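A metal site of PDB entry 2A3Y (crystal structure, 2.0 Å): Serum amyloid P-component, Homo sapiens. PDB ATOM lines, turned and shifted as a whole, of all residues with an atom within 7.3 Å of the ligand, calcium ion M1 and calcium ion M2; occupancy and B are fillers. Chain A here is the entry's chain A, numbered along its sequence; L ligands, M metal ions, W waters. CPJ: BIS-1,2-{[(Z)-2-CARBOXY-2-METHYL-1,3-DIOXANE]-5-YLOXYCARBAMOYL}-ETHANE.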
ATOM      1  N   SER A  48      12.246  32.076 -20.585  1.00  0.00           N
ATOM      2  CA  SER A  48      12.299  30.929 -21.492  1.00  0.00           C
ATOM      3  C   SER A  48      11.037  30.080 -21.365  1.00  0.00           C
ATOM      4  O   SER A  48      10.595  29.771 -20.256  1.00  0.00           O
ATOM      5  CB  SER A  48      13.525  30.071 -21.182  1.00  0.00           C
ATOM      6  OG  SER A  48      13.611  28.950 -22.048  1.00  0.00           O
ATOM      7  N   SER A  51      13.450  25.291 -23.745  1.00  0.00           N
ATOM      8  CA  SER A  51      14.901  25.341 -23.928  1.00  0.00           C
ATOM      9  C   SER A  51      15.444  23.968 -24.335  1.00  0.00           C
ATOM     10  O   SER A  51      15.281  22.980 -23.619  1.00  0.00           O
ATOM     11  CB  SER A  51      15.589  25.862 -22.670  1.00  0.00           C
ATOM     12  OG  SER A  51      16.999  25.714 -22.740  1.00  0.00           O
ATOM     13  N   ASN A  53      18.921  22.340 -25.742  1.00  0.00           N
ATOM     14  CA  ASN A  53      20.360  22.462 -25.961  1.00  0.00           C
ATOM     15  C   ASN A  53      20.956  21.115 -26.321  1.00  0.00           C
ATOM     16  O   ASN A  53      20.449  20.069 -25.894  1.00  0.00           O
ATOM     17  CB  ASN A  53      21.050  22.995 -24.690  1.00  0.00           C
ATOM     18  CG  ASN A  53      21.083  24.513 -24.621  1.00  0.00           C
ATOM     19  OD1 ASN A  53      20.293  25.203 -25.256  1.00  0.00           O
ATOM     20  ND2 ASN A  53      22.010  25.037 -23.811  1.00  0.00           N
ATOM     21  N   ASP A  58      24.740  25.848 -27.165  1.00  0.00           N
ATOM     22  CA  ASP A  58      23.720  26.623 -26.468  1.00  0.00           C
ATOM     23  C   ASP A  58      22.692  27.151 -27.461  1.00  0.00           C
ATOM     24  O   ASP A  58      23.013  27.390 -28.629  1.00  0.00           O
ATOM     25  CB  ASP A  58      24.377  27.782 -25.714  1.00  0.00           C
ATOM     26  CG  ASP A  58      23.376  28.579 -24.886  1.00  0.00           C
ATOM     27  OD1 ASP A  58      22.574  27.958 -24.173  1.00  0.00           O
ATOM     28  OD2 ASP A  58      23.335  29.827 -24.897  1.00  0.00           O
ATOM     29  N   ASN A  59      21.454  27.340 -27.001  1.00  0.00           N
ATOM     30  CA  ASN A  59      20.367  27.895 -27.809  1.00  0.00           C
ATOM     31  C   ASN A  59      20.208  27.209 -29.172  1.00  0.00           C
ATOM     32  O   ASN A  59      20.038  27.866 -30.197  1.00  0.00           O
ATOM     33  CB  ASN A  59      20.542  29.415 -27.984  1.00  0.00           C
ATOM     34  CG  ASN A  59      20.594  30.160 -26.661  1.00  0.00           C
ATOM     35  OD1 ASN A  59      20.376  29.581 -25.590  1.00  0.00           O
ATOM     36  ND2 ASN A  59      20.878  31.455 -26.720  1.00  0.00           N
ATOM     37  N   GLU A  60      20.297  25.884 -29.158  1.00  0.00           N
ATOM     38  CA  GLU A  60      20.098  25.090 -30.368  1.00  0.00           C
ATOM     39  C   GLU A  60      18.655  25.229 -30.856  1.00  0.00           C
ATOM     40  O   GLU A  60      18.409  25.414 -32.047  1.00  0.00           O
ATOM     41  CB  GLU A  60      20.442  23.624 -30.130  1.00  0.00           C
ATOM     42  CG  GLU A  60      20.530  22.769 -31.390  1.00  0.00           C
ATOM     43  CD  GLU A  60      21.595  23.239 -32.377  1.00  0.00           C
ATOM     44  OE1 GLU A  60      22.494  24.013 -31.991  1.00  0.00           O
ATOM     45  OE2 GLU A  60      21.524  22.819 -33.552  1.00  0.00           O
ATOM     46  N   LEU A  62      15.305  27.300 -29.066  1.00  0.00           N
ATOM     47  CA  LEU A  62      14.829  28.042 -27.906  1.00  0.00           C
ATOM     48  C   LEU A  62      13.626  28.900 -28.251  1.00  0.00           C
ATOM     49  O   LEU A  62      13.661  29.679 -29.200  1.00  0.00           O
ATOM     50  CB  LEU A  62      15.969  28.891 -27.327  1.00  0.00           C
ATOM     51  CG  LEU A  62      15.669  29.941 -26.253  1.00  0.00           C
ATOM     52  CD1 LEU A  62      15.226  29.276 -24.947  1.00  0.00           C
ATOM     53  CD2 LEU A  62      16.889  30.815 -26.014  1.00  0.00           C
ATOM     54  N   TYR A  64      11.577  31.871 -26.644  1.00  0.00           N
ATOM     55  CA  TYR A  64      11.910  32.884 -25.656  1.00  0.00           C
ATOM     56  C   TYR A  64      10.982  34.089 -25.758  1.00  0.00           C
ATOM     57  O   TYR A  64      10.840  34.692 -26.823  1.00  0.00           O
ATOM     58  CB  TYR A  64      13.368  33.327 -25.885  1.00  0.00           C
ATOM     59  CG  TYR A  64      14.002  34.110 -24.755  1.00  0.00           C
ATOM     60  CD1 TYR A  64      14.431  33.469 -23.582  1.00  0.00           C
ATOM     61  CD2 TYR A  64      14.218  35.483 -24.864  1.00  0.00           C
ATOM     62  CE1 TYR A  64      15.032  34.191 -22.550  1.00  0.00           C
ATOM     63  CE2 TYR A  64      14.819  36.205 -23.832  1.00  0.00           C
ATOM     64  CZ  TYR A  64      15.227  35.553 -22.686  1.00  0.00           C
ATOM     65  OH  TYR A  64      15.817  36.259 -21.669  1.00  0.00           O
ATOM     66  N   GLU A  66      10.477  37.752 -24.983  1.00  0.00           N
ATOM     67  CA  GLU A  66      11.249  38.965 -24.692  1.00  0.00           C
ATOM     68  C   GLU A  66      10.531  39.900 -23.725  1.00  0.00           C
ATOM     69  O   GLU A  66      11.101  40.395 -22.759  1.00  0.00           O
ATOM     70  CB  GLU A  66      11.526  39.727 -25.987  1.00  0.00           C
ATOM     71  CG  GLU A  66      12.169  38.921 -27.102  1.00  0.00           C
ATOM     72  CD  GLU A  66      13.637  38.648 -26.861  1.00  0.00           C
ATOM     73  OE1 GLU A  66      14.272  39.386 -26.079  1.00  0.00           O
ATOM     74  OE2 GLU A  66      14.155  37.685 -27.466  1.00  0.00           O
ATOM     75  N   TYR A  74      14.933  30.877 -31.389  1.00  0.00           N
ATOM     76  CA  TYR A  74      16.344  30.673 -31.673  1.00  0.00           C
ATOM     77  C   TYR A  74      16.513  29.328 -32.377  1.00  0.00           C
ATOM     78  O   TYR A  74      15.983  28.326 -31.910  1.00  0.00           O
ATOM     79  CB  TYR A  74      17.170  30.683 -30.388  1.00  0.00           C
ATOM     80  CG  TYR A  74      17.345  32.051 -29.750  1.00  0.00           C
ATOM     81  CD1 TYR A  74      16.296  32.667 -29.079  1.00  0.00           C
ATOM     82  CD2 TYR A  74      18.565  32.713 -29.816  1.00  0.00           C
ATOM     83  CE1 TYR A  74      16.452  33.915 -28.492  1.00  0.00           C
ATOM     84  CE2 TYR A  74      18.741  33.970 -29.232  1.00  0.00           C
ATOM     85  CZ  TYR A  74      17.670  34.564 -28.570  1.00  0.00           C
ATOM     86  OH  TYR A  74      17.829  35.791 -27.994  1.00  0.00           O
ATOM     87  N   ARG A  77      21.507  29.237 -32.327  1.00  0.00           N
ATOM     88  CA  ARG A  77      22.013  30.533 -31.864  1.00  0.00           C
ATOM     89  C   ARG A  77      21.508  31.762 -32.636  1.00  0.00           C
ATOM     90  O   ARG A  77      21.568  32.874 -32.119  1.00  0.00           O
ATOM     91  CB  ARG A  77      23.547  30.536 -31.752  1.00  0.00           C
ATOM     92  CG  ARG A  77      24.048  29.719 -30.570  1.00  0.00           C
ATOM     93  CD  ARG A  77      25.277  28.849 -30.821  1.00  0.00           C
ATOM     94  NE  ARG A  77      25.186  27.985 -32.012  1.00  0.00           N
ATOM     95  CZ  ARG A  77      24.492  26.856 -32.087  1.00  0.00           C
ATOM     96  NH1 ARG A  77      23.773  26.412 -31.063  1.00  0.00           N
ATOM     97  NH2 ARG A  77      24.502  26.154 -33.224  1.00  0.00           N
ATOM     98  N   LYS A  79      18.505  34.116 -34.210  1.00  0.00           N
ATOM     99  CA  LYS A  79      17.242  34.493 -33.589  1.00  0.00           C
ATOM    100  C   LYS A  79      16.317  35.239 -34.553  1.00  0.00           C
ATOM    101  O   LYS A  79      16.775  36.058 -35.360  1.00  0.00           O
ATOM    102  CB  LYS A  79      17.534  35.322 -32.322  1.00  0.00           C
ATOM    103  CG  LYS A  79      16.414  36.203 -31.804  1.00  0.00           C
ATOM    104  CD  LYS A  79      16.989  37.356 -30.998  1.00  0.00           C
ATOM    105  CE  LYS A  79      15.952  38.001 -30.114  1.00  0.00           C
ATOM    106  NZ  LYS A  79      16.524  38.421 -28.803  1.00  0.00           N
ATOM    107  N   GLU A 136      16.079  28.494 -18.551  1.00  0.00           N
ATOM    108  CA  GLU A 136      16.864  28.614 -19.763  1.00  0.00           C
ATOM    109  C   GLU A 136      18.244  27.975 -19.555  1.00  0.00           C
ATOM    110  O   GLU A 136      18.973  28.336 -18.627  1.00  0.00           O
ATOM    111  CB  GLU A 136      17.021  30.079 -20.166  1.00  0.00           C
ATOM    112  CG  GLU A 136      17.107  30.324 -21.672  1.00  0.00           C
ATOM    113  CD  GLU A 136      18.497  30.097 -22.233  1.00  0.00           C
ATOM    114  OE1 GLU A 136      19.484  30.538 -21.594  1.00  0.00           O
ATOM    115  OE2 GLU A 136      18.606  29.488 -23.314  1.00  0.00           O
ATOM    116  N   GLN A 137      18.594  27.028 -20.428  1.00  0.00           N
ATOM    117  CA  GLN A 137      19.894  26.372 -20.346  1.00  0.00           C
ATOM    118  C   GLN A 137      20.983  27.233 -20.981  1.00  0.00           C
ATOM    119  O   GLN A 137      20.752  27.871 -22.002  1.00  0.00           O
ATOM    120  CB  GLN A 137      19.873  25.045 -21.096  1.00  0.00           C
ATOM    121  CG  GLN A 137      19.064  23.942 -20.461  1.00  0.00           C
ATOM    122  CD  GLN A 137      18.898  22.776 -21.415  1.00  0.00           C
ATOM    123  OE1 GLN A 137      19.730  21.880 -21.456  1.00  0.00           O
ATOM    124  NE2 GLN A 137      17.831  22.808 -22.205  1.00  0.00           N
ATOM    125  N   ASP A 138      22.170  27.237 -20.374  1.00  0.00           N
ATOM    126  CA  ASP A 138      23.364  27.771 -21.021  1.00  0.00           C
ATOM    127  C   ASP A 138      24.412  26.679 -21.229  1.00  0.00           C
ATOM    128  O   ASP A 138      25.389  26.862 -21.960  1.00  0.00           O
ATOM    129  CB  ASP A 138      23.936  28.956 -20.254  1.00  0.00           C
ATOM    130  CG  ASP A 138      23.109  30.221 -20.407  1.00  0.00           C
ATOM    131  OD1 ASP A 138      22.370  30.355 -21.416  1.00  0.00           O
ATOM    132  OD2 ASP A 138      23.127  31.147 -19.570  1.00  0.00           O
ATOM    133  N   SER A 139      24.201  25.545 -20.572  1.00  0.00           N
ATOM    134  CA  SER A 139      25.033  24.359 -20.752  1.00  0.00           C
ATOM    135  C   SER A 139      24.157  23.184 -21.178  1.00  0.00           C
ATOM    136  O   SER A 139      22.940  23.335 -21.329  1.00  0.00           O
ATOM    137  CB  SER A 139      25.781  24.030 -19.463  1.00  0.00           C
ATOM    138  OG  SER A 139      24.930  23.376 -18.537  1.00  0.00           O
ATOM    139  N   GLY A 142      22.023  22.417 -17.992  1.00  0.00           N
ATOM    140  CA  GLY A 142      22.143  23.295 -16.845  1.00  0.00           C
ATOM    141  C   GLY A 142      22.581  24.719 -17.121  1.00  0.00           C
ATOM    142  O   GLY A 142      22.254  25.288 -18.173  1.00  0.00           O
ATOM    143  N   LYS A 143      23.348  25.277 -16.181  1.00  0.00           N
ATOM    144  CA  LYS A 143      23.738  26.691 -16.169  1.00  0.00           C
ATOM    145  C   LYS A 143      22.524  27.589 -16.357  1.00  0.00           C
ATOM    146  O   LYS A 143      22.436  28.375 -17.325  1.00  0.00           O
ATOM    147  CB  LYS A 143      24.856  26.975 -17.185  1.00  0.00           C
ATOM    148  CG  LYS A 143      26.254  26.557 -16.709  1.00  0.00           C
ATOM    149  CD  LYS A 143      27.347  27.130 -17.615  1.00  0.00           C
ATOM    150  CE  LYS A 143      28.643  26.338 -17.488  1.00  0.00           C
ATOM    151  NZ  LYS A 143      29.758  26.989 -18.213  1.00  0.00           N
ATOM    152  N   PHE A 144      21.580  27.456 -15.435  1.00  0.00           N
ATOM    153  CA  PHE A 144      20.316  28.186 -15.489  1.00  0.00           C
ATOM    154  C   PHE A 144      20.492  29.632 -15.019  1.00  0.00           C
ATOM    155  O   PHE A 144      21.531  29.986 -14.450  1.00  0.00           O
ATOM    156  CB  PHE A 144      19.255  27.462 -14.634  1.00  0.00           C
ATOM    157  CG  PHE A 144      18.982  26.047 -15.063  1.00  0.00           C
ATOM    158  CD1 PHE A 144      18.828  25.719 -16.415  1.00  0.00           C
ATOM    159  CD2 PHE A 144      18.855  25.033 -14.123  1.00  0.00           C
ATOM    160  CE1 PHE A 144      18.571  24.412 -16.806  1.00  0.00           C
ATOM    161  CE2 PHE A 144      18.596  23.726 -14.505  1.00  0.00           C
ATOM    162  CZ  PHE A 144      18.447  23.411 -15.854  1.00  0.00           C
ATOM    163  N   ASP A 145      19.477  30.448 -15.270  1.00  0.00           N
ATOM    164  CA  ASP A 145      19.521  31.873 -14.939  1.00  0.00           C
ATOM    165  C   ASP A 145      18.183  32.293 -14.332  1.00  0.00           C
ATOM    166  O   ASP A 145      17.142  32.237 -14.991  1.00  0.00           O
ATOM    167  CB  ASP A 145      19.840  32.689 -16.196  1.00  0.00           C
ATOM    168  CG  ASP A 145      19.993  34.189 -15.923  1.00  0.00           C
ATOM    169  OD1 ASP A 145      19.561  34.686 -14.853  1.00  0.00           O
ATOM    170  OD2 ASP A 145      20.514  34.962 -16.751  1.00  0.00           O
ATOM    171  N   GLN A 148      15.722  34.498 -16.079  1.00  0.00           N
ATOM    172  CA  GLN A 148      15.155  33.914 -17.294  1.00  0.00           C
ATOM    173  C   GLN A 148      14.177  32.771 -16.985  1.00  0.00           C
ATOM    174  O   GLN A 148      13.585  32.188 -17.894  1.00  0.00           O
ATOM    175  CB  GLN A 148      16.258  33.423 -18.227  1.00  0.00           C
ATOM    176  CG  GLN A 148      17.084  34.545 -18.876  1.00  0.00           C
ATOM    177  CD  GLN A 148      18.265  34.026 -19.680  1.00  0.00           C
ATOM    178  OE1 GLN A 148      18.875  33.013 -19.334  1.00  0.00           O
ATOM    179  NE2 GLN A 148      18.609  34.744 -20.745  1.00  0.00           N
HETATM  180  C12 CPJ L   1      22.301  39.103 -24.849  1.00  0.00           C
HETATM  181  O13 CPJ L   1      23.169  39.818 -24.374  1.00  0.00           O
HETATM  182  O11 CPJ L   1      22.395  37.658 -24.692  1.00  0.00           O
HETATM  183  C3  CPJ L   1      21.224  36.853 -24.786  1.00  0.00           C
HETATM  184  C2  CPJ L   1      21.544  35.559 -25.499  1.00  0.00           C
HETATM  185  O1  CPJ L   1      20.401  34.701 -25.520  1.00  0.00           O
HETATM  186  C4  CPJ L   1      20.737  36.501 -23.382  1.00  0.00           C
HETATM  187  O5  CPJ L   1      19.612  35.618 -23.464  1.00  0.00           O
HETATM  188  C6  CPJ L   1      19.776  34.426 -24.245  1.00  0.00           C
HETATM  189  C10 CPJ L   1      18.387  33.880 -24.530  1.00  0.00           C
HETATM  190  C7  CPJ L   1      20.553  33.374 -23.479  1.00  0.00           C
HETATM  191  O8  CPJ L   1      20.542  33.398 -22.234  1.00  0.00           O
HETATM  192  O9  CPJ L   1      21.173  32.493 -24.131  1.00  0.00           O
HETATM  193 CA    CA M   1      20.865  31.854 -20.175  1.00  0.00          CA
HETATM  194 CA    CA M   2      21.168  29.747 -23.309  1.00  0.00          CA
HETATM  195  O   HOH W   1      20.581  30.401 -18.506  1.00  0.00           O
HETATM  196  O   HOH W   2      21.674  33.790 -18.972  1.00  0.00           O
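Leu 62 touches the ligand.
Tyr 64 touches the ligand (CE1 to C10, 3.9 Å).
OH of Tyr 74 touches O1 of the ligand, 3.7 Å away.
Hydrophobic or aromatic side chains within 4 Å of the ligand: Leu 62 and Tyr 64.
Of the 21 residues printed, 8 come within 4 Å of the ligand.
The nearest printed residue that does not touch the ligand is Gln 137 (5.1 Å).
NZ of Lys 79 sits at hydrogen-bond distance from OH of Tyr 74 (3.0 Å).
The backbone carbonyl oxygen (O) of Leu 62 sits at hydrogen-bond distance from the backbone NH (N) of Tyr 74 (2.8 Å).
The side-chain amide nitrogen of Gln 148 lies within hydrogen-bond range of the side-chain hydroxyl of Tyr 64 (3.3 Å).
N of Ser 48 lies within hydrogen-bond range of O of Gln 148 (3.0 Å).
The side-chain amide oxygen (OD1) of Asn 53 sits at hydrogen-bond distance from the backbone NH (N) of Asn 59 (3.0 Å).
N of Asp 138 lies within hydrogen-bond range of O of Lys 143 (3.3 Å).
The backbone carbonyl oxygen of Asp 58 sits at hydrogen-bond distance from the guanidinium group of Arg 77 (2.7 Å).
The side-chain carboxylate of Asp 58 lies close to the side-chain amide nitrogen of Asn 53 (3.0 Å).
Calcium ion M1 is bound by water W1 (2.2 Å).
Calcium ion M1 is bound by OE1 of Glu 136, at 2.4 Å.
Calcium ion M1 is bound by water W2 (2.4 Å).
The side-chain carboxylate (OD2) of Asp 138 is bound to calcium ion M1.
The side-chain amide oxygen (OE1) of Gln 148 is bound to calcium ion M1, at 2.5 Å.
OD1 of Asp 138 is bound to calcium ion M1 (2.5 Å).
Calcium ion M1 is bound by an oxygen (O8) of the ligand, 2.6 Å away.
Water W1 lies within hydrogen-bond range of the backbone carbonyl oxygen of Glu 136, the backbone carbonyl oxygen of Lys 143 and the backbone NH of Asp 145.
Of the 21 residues printed, 3 come within 4 Å of calcium ion M1.
The nearest printed residue that does not touch calcium ion M1 is Asp 145 (4.2 Å).
Of the 21 residues printed, 5 come within 4 Å of calcium ion M2.
The nearest printed residue that does not touch calcium ion M2 is Asn 53 (4.8 Å).
OD1 of Asp 138 binds calcium ion M2 (2.3 Å).
The backbone carbonyl oxygen (O) of Gln 137 binds calcium ion M2.
Calcium ion M2 is bound by the side-chain amide oxygen (OD1) of Asn 59 (2.4 Å).
OD1 of Asp 58 binds calcium ion M2, 2.4 Å away.
The side-chain carboxylate (OE1) of Glu 136 is bound to calcium ion M2.
Calcium ion M2 is bound by the side-chain carboxylate (OE2) of Glu 136, 2.6 Å away.
Calcium ion M2 is bound by the side-chain carboxylate (OD2) of Asp 58, at 2.7 Å.
O9 of the ligand is bound to calcium ion M2, at 2.9 Å.
Calcium ion M2 has eight donor atoms within binding distance.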
